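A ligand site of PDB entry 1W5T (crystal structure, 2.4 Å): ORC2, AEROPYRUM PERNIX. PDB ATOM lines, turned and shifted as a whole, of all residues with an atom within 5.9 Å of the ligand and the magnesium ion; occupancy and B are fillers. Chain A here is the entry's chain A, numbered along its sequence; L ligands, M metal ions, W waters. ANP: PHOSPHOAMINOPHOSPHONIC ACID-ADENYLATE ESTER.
N of Thr 66 is in hydrogen-bond range of O1A of the ligand (3.4 Å).
N7 of the ligand is in hydrogen-bond range of OH of Tyr 215.
NH1 of Arg 260 is in salt-bridge range of O1G of the ligand.
The backbone NH (N) of Thr 67 sits at hydrogen-bond distance from an oxygen (O1A) of the ligand (2.8 Å).
OG1 of Thr 67 lies within hydrogen-bond range of O1A of the ligand (2.8 Å).
The backbone NH of Gly 62 lies within hydrogen-bond range of an oxygen (O3G) of the ligand.
An oxygen (O2') of the ligand is in hydrogen-bond range of the guanidinium group (NH2) of Arg 227.
O of Val 26 lies within hydrogen-bond range of N6 of the ligand, 2.9 Å away.
The backbone NH of Lys 65 sits at hydrogen-bond distance from an oxygen (O2B) of the ligand, 3.3 Å away.
O2B of the ligand is in salt-bridge range of NZ of Lys 65 (2.9 Å).
An oxygen (O3A) of the ligand is in hydrogen-bond range of the backbone NH (N) of Gly 64, 2.9 Å away.
The backbone NH (N) of Ile 63 is in hydrogen-bond range of an oxygen (O2B) of the ligand (3.1 Å).
An oxygen (O2') of the ligand sits at hydrogen-bond distance from the backbone carbonyl oxygen (O) of Tyr 19.
Within 4 Å of the magnesium ion: Thr 66.
The side-chain hydroxyl (OG1) of Thr 66 lies close to the side-chain carboxylate (OD2) of Asp 145 (2.8 Å).
The side-chain hydroxyl (OH) of Tyr 215 sits at hydrogen-bond distance from the backbone carbonyl oxygen (O) of Ile 63.
The backbone carbonyl oxygen (O) of Gly 62 lies within hydrogen-bond range of the backbone NH (N) of Ala 259, 2.8 Å away.
The side-chain amide nitrogen (NE2) of Gln 226 lies within hydrogen-bond range of the backbone carbonyl oxygen (O) of Glu 23.
The magnesium ion is bound by water W4 (2.1 Å), O1B of the ligand (2.2 Å), water W3 (2.2 Å), OG1 of Thr 66 (2.3 Å) and O2G of the ligand (2.3 Å).
The magnesium ion has five donor atoms within binding distance.
Merely in contact with the ligand: Val 61, Ala 259, Leu 24, Ile 263, Ile 223, Gln 226, Arg 60, Pro 21, Glu 17 and Arg 27.
Hydrophobic or aromatic side chains within 4 Å of the ligand: Pro 21, Leu 24, Val 26, Val 61, Ile 63, Tyr 215, Ile 223, Ala 259 and Ile 263.
The nearest printed residue that does not touch the ligand is Glu 146 (4.1 Å).
Water W2 lies within hydrogen-bond range of the backbone carbonyl oxygen of Tyr 19, the guanidinium group of Arg 227, an oxygen (O3') of the ligand and the backbone carbonyl oxygen of Asp 16.
Water W1 lies within hydrogen-bond range of N of Arg 25 (2.5 Å), OE1 of Gln 226 (2.8 Å), N1 of the ligand (2.9 Å) and N of Val 26 (3.5 Å).
Water W5 lies within hydrogen-bond range of the side-chain amide oxygen (OE1) of Gln 226 (2.6 Å), the guanidinium group (NE) of Arg 227 (2.7 Å) and the backbone carbonyl oxygen (O) of Ile 223 (3.0 Å).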
ATOM      1  N   ASP A  16     -17.767  13.975  16.239  1.00  0.00           N
ATOM      2  CA  ASP A  16     -16.517  13.248  15.992  1.00  0.00           C
ATOM      3  C   ASP A  16     -16.749  12.143  14.952  1.00  0.00           C
ATOM      4  O   ASP A  16     -17.842  11.584  14.851  1.00  0.00           O
ATOM      5  CB  ASP A  16     -15.927  12.699  17.299  1.00  0.00           C
ATOM      6  CG  ASP A  16     -15.364  13.795  18.234  1.00  0.00           C
ATOM      7  OD1 ASP A  16     -15.618  15.021  18.017  1.00  0.00           O
ATOM      8  OD2 ASP A  16     -14.623  13.538  19.193  1.00  0.00           O
ATOM      9  N   GLU A  17     -15.698  11.841  14.198  1.00  0.00           N
ATOM     10  CA  GLU A  17     -15.700  10.945  13.027  1.00  0.00           C
ATOM     11  C   GLU A  17     -16.109   9.492  13.319  1.00  0.00           C
ATOM     12  O   GLU A  17     -16.688   8.806  12.473  1.00  0.00           O
ATOM     13  CB  GLU A  17     -14.320  10.998  12.349  1.00  0.00           C
ATOM     14  CG  GLU A  17     -13.424  12.091  12.944  1.00  0.00           C
ATOM     15  CD  GLU A  17     -12.278  12.565  12.057  1.00  0.00           C
ATOM     16  OE1 GLU A  17     -12.157  13.803  11.849  1.00  0.00           O
ATOM     17  OE2 GLU A  17     -11.490  11.697  11.581  1.00  0.00           O
ATOM     18  N   ASN A  18     -15.836   9.005  14.521  1.00  0.00           N
ATOM     19  CA  ASN A  18     -16.381   7.701  14.811  1.00  0.00           C
ATOM     20  C   ASN A  18     -17.550   7.668  15.783  1.00  0.00           C
ATOM     21  O   ASN A  18     -17.812   6.624  16.421  1.00  0.00           O
ATOM     22  CB  ASN A  18     -15.306   6.673  15.150  1.00  0.00           C
ATOM     23  CG  ASN A  18     -14.253   7.198  16.035  1.00  0.00           C
ATOM     24  OD1 ASN A  18     -14.516   7.602  17.177  1.00  0.00           O
ATOM     25  ND2 ASN A  18     -13.023   7.196  15.521  1.00  0.00           N
ATOM     26  N   TYR A  19     -18.278   8.780  15.900  1.00  0.00           N
ATOM     27  CA  TYR A  19     -19.514   8.714  16.612  1.00  0.00           C
ATOM     28  C   TYR A  19     -20.515   7.929  15.770  1.00  0.00           C
ATOM     29  O   TYR A  19     -20.669   8.175  14.563  1.00  0.00           O
ATOM     30  CB  TYR A  19     -20.048  10.109  16.901  1.00  0.00           C
ATOM     31  CG  TYR A  19     -21.429  10.119  17.473  1.00  0.00           C
ATOM     32  CD1 TYR A  19     -21.651   9.893  18.843  1.00  0.00           C
ATOM     33  CD2 TYR A  19     -22.542  10.337  16.644  1.00  0.00           C
ATOM     34  CE1 TYR A  19     -22.950   9.912  19.389  1.00  0.00           C
ATOM     35  CE2 TYR A  19     -23.830  10.355  17.161  1.00  0.00           C
ATOM     36  CZ  TYR A  19     -24.036  10.152  18.529  1.00  0.00           C
ATOM     37  OH  TYR A  19     -25.319  10.158  19.041  1.00  0.00           O
ATOM     38  N   ILE A  20     -21.174   6.977  16.418  1.00  0.00           N
ATOM     39  CA  ILE A  20     -22.270   6.192  15.824  1.00  0.00           C
ATOM     40  C   ILE A  20     -23.576   6.590  16.487  1.00  0.00           C
ATOM     41  O   ILE A  20     -23.719   6.514  17.705  1.00  0.00           O
ATOM     42  CB  ILE A  20     -22.030   4.673  16.079  1.00  0.00           C
ATOM     43  CG1 ILE A  20     -20.578   4.260  15.672  1.00  0.00           C
ATOM     44  CG2 ILE A  20     -23.076   3.850  15.337  1.00  0.00           C
ATOM     45  CD1 ILE A  20     -20.301   4.321  14.136  1.00  0.00           C
ATOM     46  N   PRO A  21     -24.541   7.063  15.705  1.00  0.00           N
ATOM     47  CA  PRO A  21     -25.790   7.530  16.308  1.00  0.00           C
ATOM     48  C   PRO A  21     -26.557   6.365  16.922  1.00  0.00           C
ATOM     49  O   PRO A  21     -26.336   5.252  16.478  1.00  0.00           O
ATOM     50  CB  PRO A  21     -26.515   8.246  15.143  1.00  0.00           C
ATOM     51  CG  PRO A  21     -25.805   7.894  13.957  1.00  0.00           C
ATOM     52  CD  PRO A  21     -24.490   7.292  14.258  1.00  0.00           C
ATOM     53  N   GLU A  23     -29.554   5.501  16.578  1.00  0.00           N
ATOM     54  CA  GLU A  23     -30.462   4.950  15.571  1.00  0.00           C
ATOM     55  C   GLU A  23     -30.034   5.421  14.207  1.00  0.00           C
ATOM     56  O   GLU A  23     -29.416   6.470  14.118  1.00  0.00           O
ATOM     57  CB  GLU A  23     -31.911   5.429  15.826  1.00  0.00           C
ATOM     58  CG  GLU A  23     -32.702   4.440  16.698  1.00  0.00           C
ATOM     59  CD  GLU A  23     -34.211   4.545  16.515  1.00  0.00           C
ATOM     60  OE1 GLU A  23     -34.650   5.623  16.030  1.00  0.00           O
ATOM     61  OE2 GLU A  23     -34.959   3.574  16.865  1.00  0.00           O
ATOM     62  N   LEU A  24     -30.368   4.692  13.150  1.00  0.00           N
ATOM     63  CA  LEU A  24     -30.165   5.228  11.790  1.00  0.00           C
ATOM     64  C   LEU A  24     -31.473   5.734  11.193  1.00  0.00           C
ATOM     65  O   LEU A  24     -32.493   5.077  11.301  1.00  0.00           O
ATOM     66  CB  LEU A  24     -29.558   4.211  10.841  1.00  0.00           C
ATOM     67  CG  LEU A  24     -28.073   3.814  10.964  1.00  0.00           C
ATOM     68  CD1 LEU A  24     -27.671   2.891   9.806  1.00  0.00           C
ATOM     69  CD2 LEU A  24     -27.149   4.980  11.067  1.00  0.00           C
ATOM     70  N   ARG A  25     -31.433   6.881  10.521  1.00  0.00           N
ATOM     71  CA  ARG A  25     -32.642   7.419   9.896  1.00  0.00           C
ATOM     72  C   ARG A  25     -32.595   7.409   8.356  1.00  0.00           C
ATOM     73  O   ARG A  25     -33.572   7.714   7.669  1.00  0.00           O
ATOM     74  CB  ARG A  25     -32.911   8.841  10.408  1.00  0.00           C
ATOM     75  CG  ARG A  25     -33.226   8.925  11.883  1.00  0.00           C
ATOM     76  CD  ARG A  25     -34.020  10.128  12.250  1.00  0.00           C
ATOM     77  NE  ARG A  25     -34.010  10.369  13.702  1.00  0.00           N
ATOM     78  CZ  ARG A  25     -33.988  11.562  14.268  1.00  0.00           C
ATOM     79  NH1 ARG A  25     -33.975  12.663  13.521  1.00  0.00           N
ATOM     80  NH2 ARG A  25     -34.005  11.656  15.593  1.00  0.00           N
ATOM     81  N   VAL A  26     -31.422   7.100   7.855  1.00  0.00           N
ATOM     82  CA  VAL A  26     -31.156   6.884   6.467  1.00  0.00           C
ATOM     83  C   VAL A  26     -30.323   5.615   6.515  1.00  0.00           C
ATOM     84  O   VAL A  26     -29.510   5.459   7.409  1.00  0.00           O
ATOM     85  CB  VAL A  26     -30.334   8.036   5.859  1.00  0.00           C
ATOM     86  CG1 VAL A  26     -30.116   7.784   4.349  1.00  0.00           C
ATOM     87  CG2 VAL A  26     -31.002   9.410   6.110  1.00  0.00           C
ATOM     88  N   ARG A  27     -30.549   4.712   5.561  1.00  0.00           N
ATOM     89  CA  ARG A  27     -29.913   3.375   5.503  1.00  0.00           C
ATOM     90  C   ARG A  27     -30.439   2.398   6.613  1.00  0.00           C
ATOM     91  O   ARG A  27     -29.828   1.340   6.899  1.00  0.00           O
ATOM     92  CB  ARG A  27     -28.373   3.489   5.427  1.00  0.00           C
ATOM     93  CG  ARG A  27     -27.835   4.450   4.328  1.00  0.00           C
ATOM     94  CD  ARG A  27     -28.303   4.124   2.846  1.00  0.00           C
ATOM     95  NE  ARG A  27     -27.770   5.080   1.863  1.00  0.00           N
ATOM     96  CZ  ARG A  27     -28.506   5.820   1.031  1.00  0.00           C
ATOM     97  NH1 ARG A  27     -29.846   5.739   1.007  1.00  0.00           N
ATOM     98  NH2 ARG A  27     -27.899   6.657   0.208  1.00  0.00           N
ATOM     99  N   ARG A  60     -16.215   7.627  -4.275  1.00  0.00           N
ATOM    100  CA  ARG A  60     -16.986   8.391  -3.288  1.00  0.00           C
ATOM    101  C   ARG A  60     -16.530   8.058  -1.880  1.00  0.00           C
ATOM    102  O   ARG A  60     -16.256   6.885  -1.570  1.00  0.00           O
ATOM    103  CB  ARG A  60     -18.502   8.140  -3.404  1.00  0.00           C
ATOM    104  CG  ARG A  60     -19.124   8.491  -4.753  1.00  0.00           C
ATOM    105  CD  ARG A  60     -18.920   9.982  -5.208  1.00  0.00           C
ATOM    106  NE  ARG A  60     -19.706  10.262  -6.404  1.00  0.00           N
ATOM    107  CZ  ARG A  60     -20.617  11.216  -6.527  1.00  0.00           C
ATOM    108  NH1 ARG A  60     -21.285  11.327  -7.686  1.00  0.00           N
ATOM    109  NH2 ARG A  60     -20.850  12.058  -5.519  1.00  0.00           N
ATOM    110  N   VAL A  61     -16.431   9.087  -1.031  1.00  0.00           N
ATOM    111  CA  VAL A  61     -16.053   8.923   0.382  1.00  0.00           C
ATOM    112  C   VAL A  61     -17.086   9.566   1.336  1.00  0.00           C
ATOM    113  O   VAL A  61     -17.789  10.510   0.961  1.00  0.00           O
ATOM    114  CB  VAL A  61     -14.611   9.458   0.692  1.00  0.00           C
ATOM    115  CG1 VAL A  61     -13.548   8.816  -0.192  1.00  0.00           C
ATOM    116  CG2 VAL A  61     -14.512  10.977   0.527  1.00  0.00           C
ATOM    117  N   GLY A  62     -17.201   9.044   2.555  1.00  0.00           N
ATOM    118  CA  GLY A  62     -18.071   9.619   3.561  1.00  0.00           C
ATOM    119  C   GLY A  62     -19.544   9.295   3.341  1.00  0.00           C
ATOM    120  O   GLY A  62     -20.424  10.087   3.667  1.00  0.00           O
ATOM    121  N   ILE A  63     -19.791   8.125   2.783  1.00  0.00           N
ATOM    122  CA  ILE A  63     -21.150   7.701   2.431  1.00  0.00           C
ATOM    123  C   ILE A  63     -21.711   6.574   3.307  1.00  0.00           C
ATOM    124  O   ILE A  63     -22.709   5.937   2.954  1.00  0.00           O
ATOM    125  CB  ILE A  63     -21.233   7.326   0.941  1.00  0.00           C
ATOM    126  CG1 ILE A  63     -20.211   6.234   0.620  1.00  0.00           C
ATOM    127  CG2 ILE A  63     -20.980   8.569   0.082  1.00  0.00           C
ATOM    128  CD1 ILE A  63     -20.098   5.920  -0.854  1.00  0.00           C
ATOM    129  N   GLY A  64     -21.071   6.326   4.461  1.00  0.00           N
ATOM    130  CA  GLY A  64     -21.660   5.466   5.476  1.00  0.00           C
ATOM    131  C   GLY A  64     -21.246   4.006   5.495  1.00  0.00           C
ATOM    132  O   GLY A  64     -21.821   3.236   6.237  1.00  0.00           O
ATOM    133  N   LYS A  65     -20.237   3.628   4.729  1.00  0.00           N
ATOM    134  CA  LYS A  65     -19.705   2.275   4.735  1.00  0.00           C
ATOM    135  C   LYS A  65     -19.363   1.781   6.155  1.00  0.00           C
ATOM    136  O   LYS A  65     -19.882   0.733   6.624  1.00  0.00           O
ATOM    137  CB  LYS A  65     -18.474   2.155   3.827  1.00  0.00           C
ATOM    138  CG  LYS A  65     -18.801   2.242   2.351  1.00  0.00           C
ATOM    139  CD  LYS A  65     -17.572   2.108   1.459  1.00  0.00           C
ATOM    140  CE  LYS A  65     -16.469   3.133   1.719  1.00  0.00           C
ATOM    141  NZ  LYS A  65     -16.677   4.487   1.079  1.00  0.00           N
ATOM    142  N   THR A  66     -18.500   2.530   6.823  1.00  0.00           N
ATOM    143  CA  THR A  66     -18.059   2.177   8.163  1.00  0.00           C
ATOM    144  C   THR A  66     -19.193   2.244   9.180  1.00  0.00           C
ATOM    145  O   THR A  66     -19.381   1.323   9.955  1.00  0.00           O
ATOM    146  CB  THR A  66     -16.846   3.055   8.564  1.00  0.00           C
ATOM    147  OG1 THR A  66     -15.787   2.831   7.632  1.00  0.00           O
ATOM    148  CG2 THR A  66     -16.253   2.609   9.879  1.00  0.00           C
ATOM    149  N   THR A  67     -19.937   3.347   9.155  1.00  0.00           N
ATOM    150  CA  THR A  67     -21.094   3.552  10.040  1.00  0.00           C
ATOM    151  C   THR A  67     -22.149   2.467   9.905  1.00  0.00           C
ATOM    152  O   THR A  67     -22.631   1.988  10.888  1.00  0.00           O
ATOM    153  CB  THR A  67     -21.721   4.926   9.752  1.00  0.00           C
ATOM    154  OG1 THR A  67     -20.790   5.928  10.154  1.00  0.00           O
ATOM    155  CG2 THR A  67     -22.967   5.179  10.671  1.00  0.00           C
ATOM    156  N   LEU A  68     -22.543   2.134   8.691  1.00  0.00           N
ATOM    157  CA  LEU A  68     -23.493   1.047   8.475  1.00  0.00           C
ATOM    158  C   LEU A  68     -22.979  -0.251   9.066  1.00  0.00           C
ATOM    159  O   LEU A  68     -23.730  -0.990   9.696  1.00  0.00           O
ATOM    160  CB  LEU A  68     -23.765   0.815   6.985  1.00  0.00           C
ATOM    161  CG  LEU A  68     -24.824  -0.256   6.658  1.00  0.00           C
ATOM    162  CD1 LEU A  68     -26.161  -0.012   7.401  1.00  0.00           C
ATOM    163  CD2 LEU A  68     -25.025  -0.402   5.119  1.00  0.00           C
ATOM    164  N   TYR A  91     -13.646  -4.970  15.397  1.00  0.00           N
ATOM    165  CA  TYR A  91     -13.517  -4.077  14.271  1.00  0.00           C
ATOM    166  C   TYR A  91     -12.065  -3.967  13.881  1.00  0.00           C
ATOM    167  O   TYR A  91     -11.209  -3.664  14.685  1.00  0.00           O
ATOM    168  CB  TYR A  91     -14.132  -2.694  14.553  1.00  0.00           C
ATOM    169  CG  TYR A  91     -13.915  -1.734  13.406  1.00  0.00           C
ATOM    170  CD1 TYR A  91     -14.748  -1.757  12.260  1.00  0.00           C
ATOM    171  CD2 TYR A  91     -12.871  -0.858  13.443  1.00  0.00           C
ATOM    172  CE1 TYR A  91     -14.511  -0.868  11.172  1.00  0.00           C
ATOM    173  CE2 TYR A  91     -12.586  -0.027  12.387  1.00  0.00           C
ATOM    174  CZ  TYR A  91     -13.397  -0.002  11.267  1.00  0.00           C
ATOM    175  OH  TYR A  91     -13.066   0.881  10.293  1.00  0.00           O
ATOM    176  N   ASP A 145     -12.863  -3.869   7.730  1.00  0.00           N
ATOM    177  CA  ASP A 145     -12.892  -2.626   6.967  1.00  0.00           C
ATOM    178  C   ASP A 145     -11.702  -2.431   6.035  1.00  0.00           C
ATOM    179  O   ASP A 145     -10.611  -2.965   6.270  1.00  0.00           O
ATOM    180  CB  ASP A 145     -12.959  -1.436   7.925  1.00  0.00           C
ATOM    181  CG  ASP A 145     -13.807  -0.296   7.410  1.00  0.00           C
ATOM    182  OD1 ASP A 145     -14.118  -0.226   6.191  1.00  0.00           O
ATOM    183  OD2 ASP A 145     -14.227   0.583   8.171  1.00  0.00           O
ATOM    184  N   GLU A 146     -11.914  -1.636   4.995  1.00  0.00           N
ATOM    185  CA  GLU A 146     -10.903  -1.417   3.963  1.00  0.00           C
ATOM    186  C   GLU A 146     -10.413  -2.777   3.490  1.00  0.00           C
ATOM    187  O   GLU A 146      -9.207  -2.977   3.355  1.00  0.00           O
ATOM    188  CB  GLU A 146      -9.706  -0.579   4.476  1.00  0.00           C
ATOM    189  CG  GLU A 146     -10.028   0.800   5.051  1.00  0.00           C
ATOM    190  CD  GLU A 146     -10.493   1.819   4.010  1.00  0.00           C
ATOM    191  OE1 GLU A 146     -10.875   2.937   4.382  1.00  0.00           O
ATOM    192  OE2 GLU A 146     -10.477   1.526   2.809  1.00  0.00           O
ATOM    193  N   VAL A 185     -15.962  -4.749   4.589  1.00  0.00           N
ATOM    194  CA  VAL A 185     -16.306  -3.421   4.049  1.00  0.00           C
ATOM    195  C   VAL A 185     -15.198  -2.994   3.117  1.00  0.00           C
ATOM    196  O   VAL A 185     -14.084  -2.945   3.576  1.00  0.00           O
ATOM    197  CB  VAL A 185     -16.442  -2.404   5.182  1.00  0.00           C
ATOM    198  CG1 VAL A 185     -16.800  -1.014   4.635  1.00  0.00           C
ATOM    199  CG2 VAL A 185     -17.465  -2.867   6.211  1.00  0.00           C
ATOM    200  N   TYR A 215     -25.076  10.229  -0.961  1.00  0.00           N
ATOM    201  CA  TYR A 215     -26.319  10.764  -0.428  1.00  0.00           C
ATOM    202  C   TYR A 215     -26.949  11.921  -1.213  1.00  0.00           C
ATOM    203  O   TYR A 215     -26.275  12.906  -1.612  1.00  0.00           O
ATOM    204  CB  TYR A 215     -26.083  11.219   1.029  1.00  0.00           C
ATOM    205  CG  TYR A 215     -25.839  10.083   2.007  1.00  0.00           C
ATOM    206  CD1 TYR A 215     -24.602   9.973   2.675  1.00  0.00           C
ATOM    207  CD2 TYR A 215     -26.853   9.139   2.288  1.00  0.00           C
ATOM    208  CE1 TYR A 215     -24.384   8.938   3.590  1.00  0.00           C
ATOM    209  CE2 TYR A 215     -26.634   8.086   3.211  1.00  0.00           C
ATOM    210  CZ  TYR A 215     -25.398   7.991   3.837  1.00  0.00           C
ATOM    211  OH  TYR A 215     -25.212   6.986   4.727  1.00  0.00           O
ATOM    212  N   ILE A 223     -29.786  13.478   7.857  1.00  0.00           N
ATOM    213  CA  ILE A 223     -28.581  13.184   8.663  1.00  0.00           C
ATOM    214  C   ILE A 223     -28.129  14.371   9.536  1.00  0.00           C
ATOM    215  O   ILE A 223     -27.757  14.176  10.703  1.00  0.00           O
ATOM    216  CB  ILE A 223     -27.421  12.604   7.799  1.00  0.00           C
ATOM    217  CG1 ILE A 223     -27.847  11.253   7.198  1.00  0.00           C
ATOM    218  CG2 ILE A 223     -26.091  12.537   8.641  1.00  0.00           C
ATOM    219  CD1 ILE A 223     -26.926  10.716   6.014  1.00  0.00           C
ATOM    220  N   GLN A 226     -30.644  14.931  12.678  1.00  0.00           N
ATOM    221  CA  GLN A 226     -30.256  14.038  13.752  1.00  0.00           C
ATOM    222  C   GLN A 226     -28.963  14.484  14.471  1.00  0.00           C
ATOM    223  O   GLN A 226     -28.925  14.462  15.691  1.00  0.00           O
ATOM    224  CB  GLN A 226     -30.133  12.596  13.207  1.00  0.00           C
ATOM    225  CG  GLN A 226     -29.697  11.552  14.222  1.00  0.00           C
ATOM    226  CD  GLN A 226     -29.562  10.175  13.622  1.00  0.00           C
ATOM    227  OE1 GLN A 226     -28.867   9.994  12.606  1.00  0.00           O
ATOM    228  NE2 GLN A 226     -30.202   9.174  14.252  1.00  0.00           N
ATOM    229  N   ARG A 227     -27.926  14.909  13.753  1.00  0.00           N
ATOM    230  CA  ARG A 227     -26.772  15.480  14.467  1.00  0.00           C
ATOM    231  C   ARG A 227     -27.143  16.763  15.289  1.00  0.00           C
ATOM    232  O   ARG A 227     -26.753  16.921  16.455  1.00  0.00           O
ATOM    233  CB  ARG A 227     -25.582  15.753  13.539  1.00  0.00           C
ATOM    234  CG  ARG A 227     -24.773  14.549  13.064  1.00  0.00           C
ATOM    235  CD  ARG A 227     -24.750  13.277  13.963  1.00  0.00           C
ATOM    236  NE  ARG A 227     -24.482  12.143  13.107  1.00  0.00           N
ATOM    237  CZ  ARG A 227     -23.312  11.543  12.997  1.00  0.00           C
ATOM    238  NH1 ARG A 227     -22.264  11.931  13.747  1.00  0.00           N
ATOM    239  NH2 ARG A 227     -23.178  10.521  12.131  1.00  0.00           N
ATOM    240  N   ALA A 259     -21.723  12.539   3.580  1.00  0.00           N
ATOM    241  CA  ALA A 259     -22.183  12.898   4.920  1.00  0.00           C
ATOM    242  C   ALA A 259     -21.079  13.416   5.853  1.00  0.00           C
ATOM    243  O   ALA A 259     -21.314  14.309   6.701  1.00  0.00           O
ATOM    244  CB  ALA A 259     -22.978  11.747   5.574  1.00  0.00           C
ATOM    245  N   ARG A 260     -19.882  12.899   5.699  1.00  0.00           N
ATOM    246  CA  ARG A 260     -18.731  13.430   6.450  1.00  0.00           C
ATOM    247  C   ARG A 260     -18.577  14.929   6.202  1.00  0.00           C
ATOM    248  O   ARG A 260     -18.471  15.698   7.132  1.00  0.00           O
ATOM    249  CB  ARG A 260     -17.420  12.695   6.095  1.00  0.00           C
ATOM    250  CG  ARG A 260     -16.135  13.441   6.450  1.00  0.00           C
ATOM    251  CD  ARG A 260     -15.042  12.571   7.095  1.00  0.00           C
ATOM    252  NE  ARG A 260     -14.900  11.292   6.367  1.00  0.00           N
ATOM    253  CZ  ARG A 260     -14.879  10.076   6.942  1.00  0.00           C
ATOM    254  NH1 ARG A 260     -14.752   9.013   6.159  1.00  0.00           N
ATOM    255  NH2 ARG A 260     -14.973   9.904   8.278  1.00  0.00           N
ATOM    256  N   ILE A 263     -21.536  17.029   7.784  1.00  0.00           N
ATOM    257  CA  ILE A 263     -21.431  17.096   9.218  1.00  0.00           C
ATOM    258  C   ILE A 263     -20.298  18.021   9.693  1.00  0.00           C
ATOM    259  O   ILE A 263     -20.476  18.753  10.687  1.00  0.00           O
ATOM    260  CB  ILE A 263     -21.273  15.671   9.807  1.00  0.00           C
ATOM    261  CG1 ILE A 263     -22.602  14.941   9.727  1.00  0.00           C
ATOM    262  CG2 ILE A 263     -20.839  15.697  11.263  1.00  0.00           C
ATOM    263  CD1 ILE A 263     -22.444  13.465   9.872  1.00  0.00           C
HETATM  264  PG  ANP L   1     -14.635   6.766   3.548  1.00  0.00           P
HETATM  265  O1G ANP L   1     -13.564   7.891   3.894  1.00  0.00           O
HETATM  266  O2G ANP L   1     -14.140   5.410   4.211  1.00  0.00           O
HETATM  267  O3G ANP L   1     -14.867   6.589   1.996  1.00  0.00           O
HETATM  268  PB  ANP L   1     -17.296   6.072   4.712  1.00  0.00           P
HETATM  269  O1B ANP L   1     -16.803   4.786   5.486  1.00  0.00           O
HETATM  270  O2B ANP L   1     -18.005   5.625   3.391  1.00  0.00           O
HETATM  271  N3B ANP L   1     -16.059   7.210   4.396  1.00  0.00           N
HETATM  272  PA  ANP L   1     -18.534   6.930   7.162  1.00  0.00           P
HETATM  273  O1A ANP L   1     -19.370   5.670   7.702  1.00  0.00           O
HETATM  274  O2A ANP L   1     -17.136   6.981   7.907  1.00  0.00           O
HETATM  275  O3A ANP L   1     -18.408   6.911   5.555  1.00  0.00           O
HETATM  276  O5' ANP L   1     -19.400   8.276   7.348  1.00  0.00           O
HETATM  277  C5' ANP L   1     -19.027   9.650   7.187  1.00  0.00           C
HETATM  278  C4' ANP L   1     -19.734  10.413   8.307  1.00  0.00           C
HETATM  279  O4' ANP L   1     -21.146  10.463   8.073  1.00  0.00           O
HETATM  280  C3' ANP L   1     -19.616   9.727   9.669  1.00  0.00           C
HETATM  281  O3' ANP L   1     -19.596  10.717  10.649  1.00  0.00           O
HETATM  282  C2' ANP L   1     -20.906   8.927   9.818  1.00  0.00           C
HETATM  283  O2' ANP L   1     -21.302   8.622  11.154  1.00  0.00           O
HETATM  284  C1' ANP L   1     -21.896   9.850   9.117  1.00  0.00           C
HETATM  285  N9  ANP L   1     -22.932   9.059   8.448  1.00  0.00           N
HETATM  286  C8  ANP L   1     -22.788   8.412   7.232  1.00  0.00           C
HETATM  287  N7  ANP L   1     -23.922   7.767   6.869  1.00  0.00           N
HETATM  288  C5  ANP L   1     -24.849   8.004   7.819  1.00  0.00           C
HETATM  289  C6  ANP L   1     -26.261   7.679   8.159  1.00  0.00           C
HETATM  290  N6  ANP L   1     -27.052   6.912   7.356  1.00  0.00           N
HETATM  291  N1  ANP L   1     -26.796   8.139   9.322  1.00  0.00           N
HETATM  292  C2  ANP L   1     -26.116   8.893  10.174  1.00  0.00           C
HETATM  293  N3  ANP L   1     -24.819   9.242   9.994  1.00  0.00           N
HETATM  294  C4  ANP L   1     -24.158   8.821   8.813  1.00  0.00           C
HETATM  295 MG    MG M   1     -14.833   4.090   6.008  1.00  0.00          MG
HETATM  296  O   HOH W   1     -29.433   8.428  10.370  1.00  0.00           O
HETATM  297  O   HOH W   2     -20.065  10.450  13.294  1.00  0.00           O
HETATM  298  O   HOH W   3     -14.931   5.538   7.663  1.00  0.00           O
HETATM  299  O   HOH W   4     -14.508   2.255   4.940  1.00  0.00           O
HETATM  300  O   HOH W   5     -26.915  11.635  11.980  1.00  0.00           O
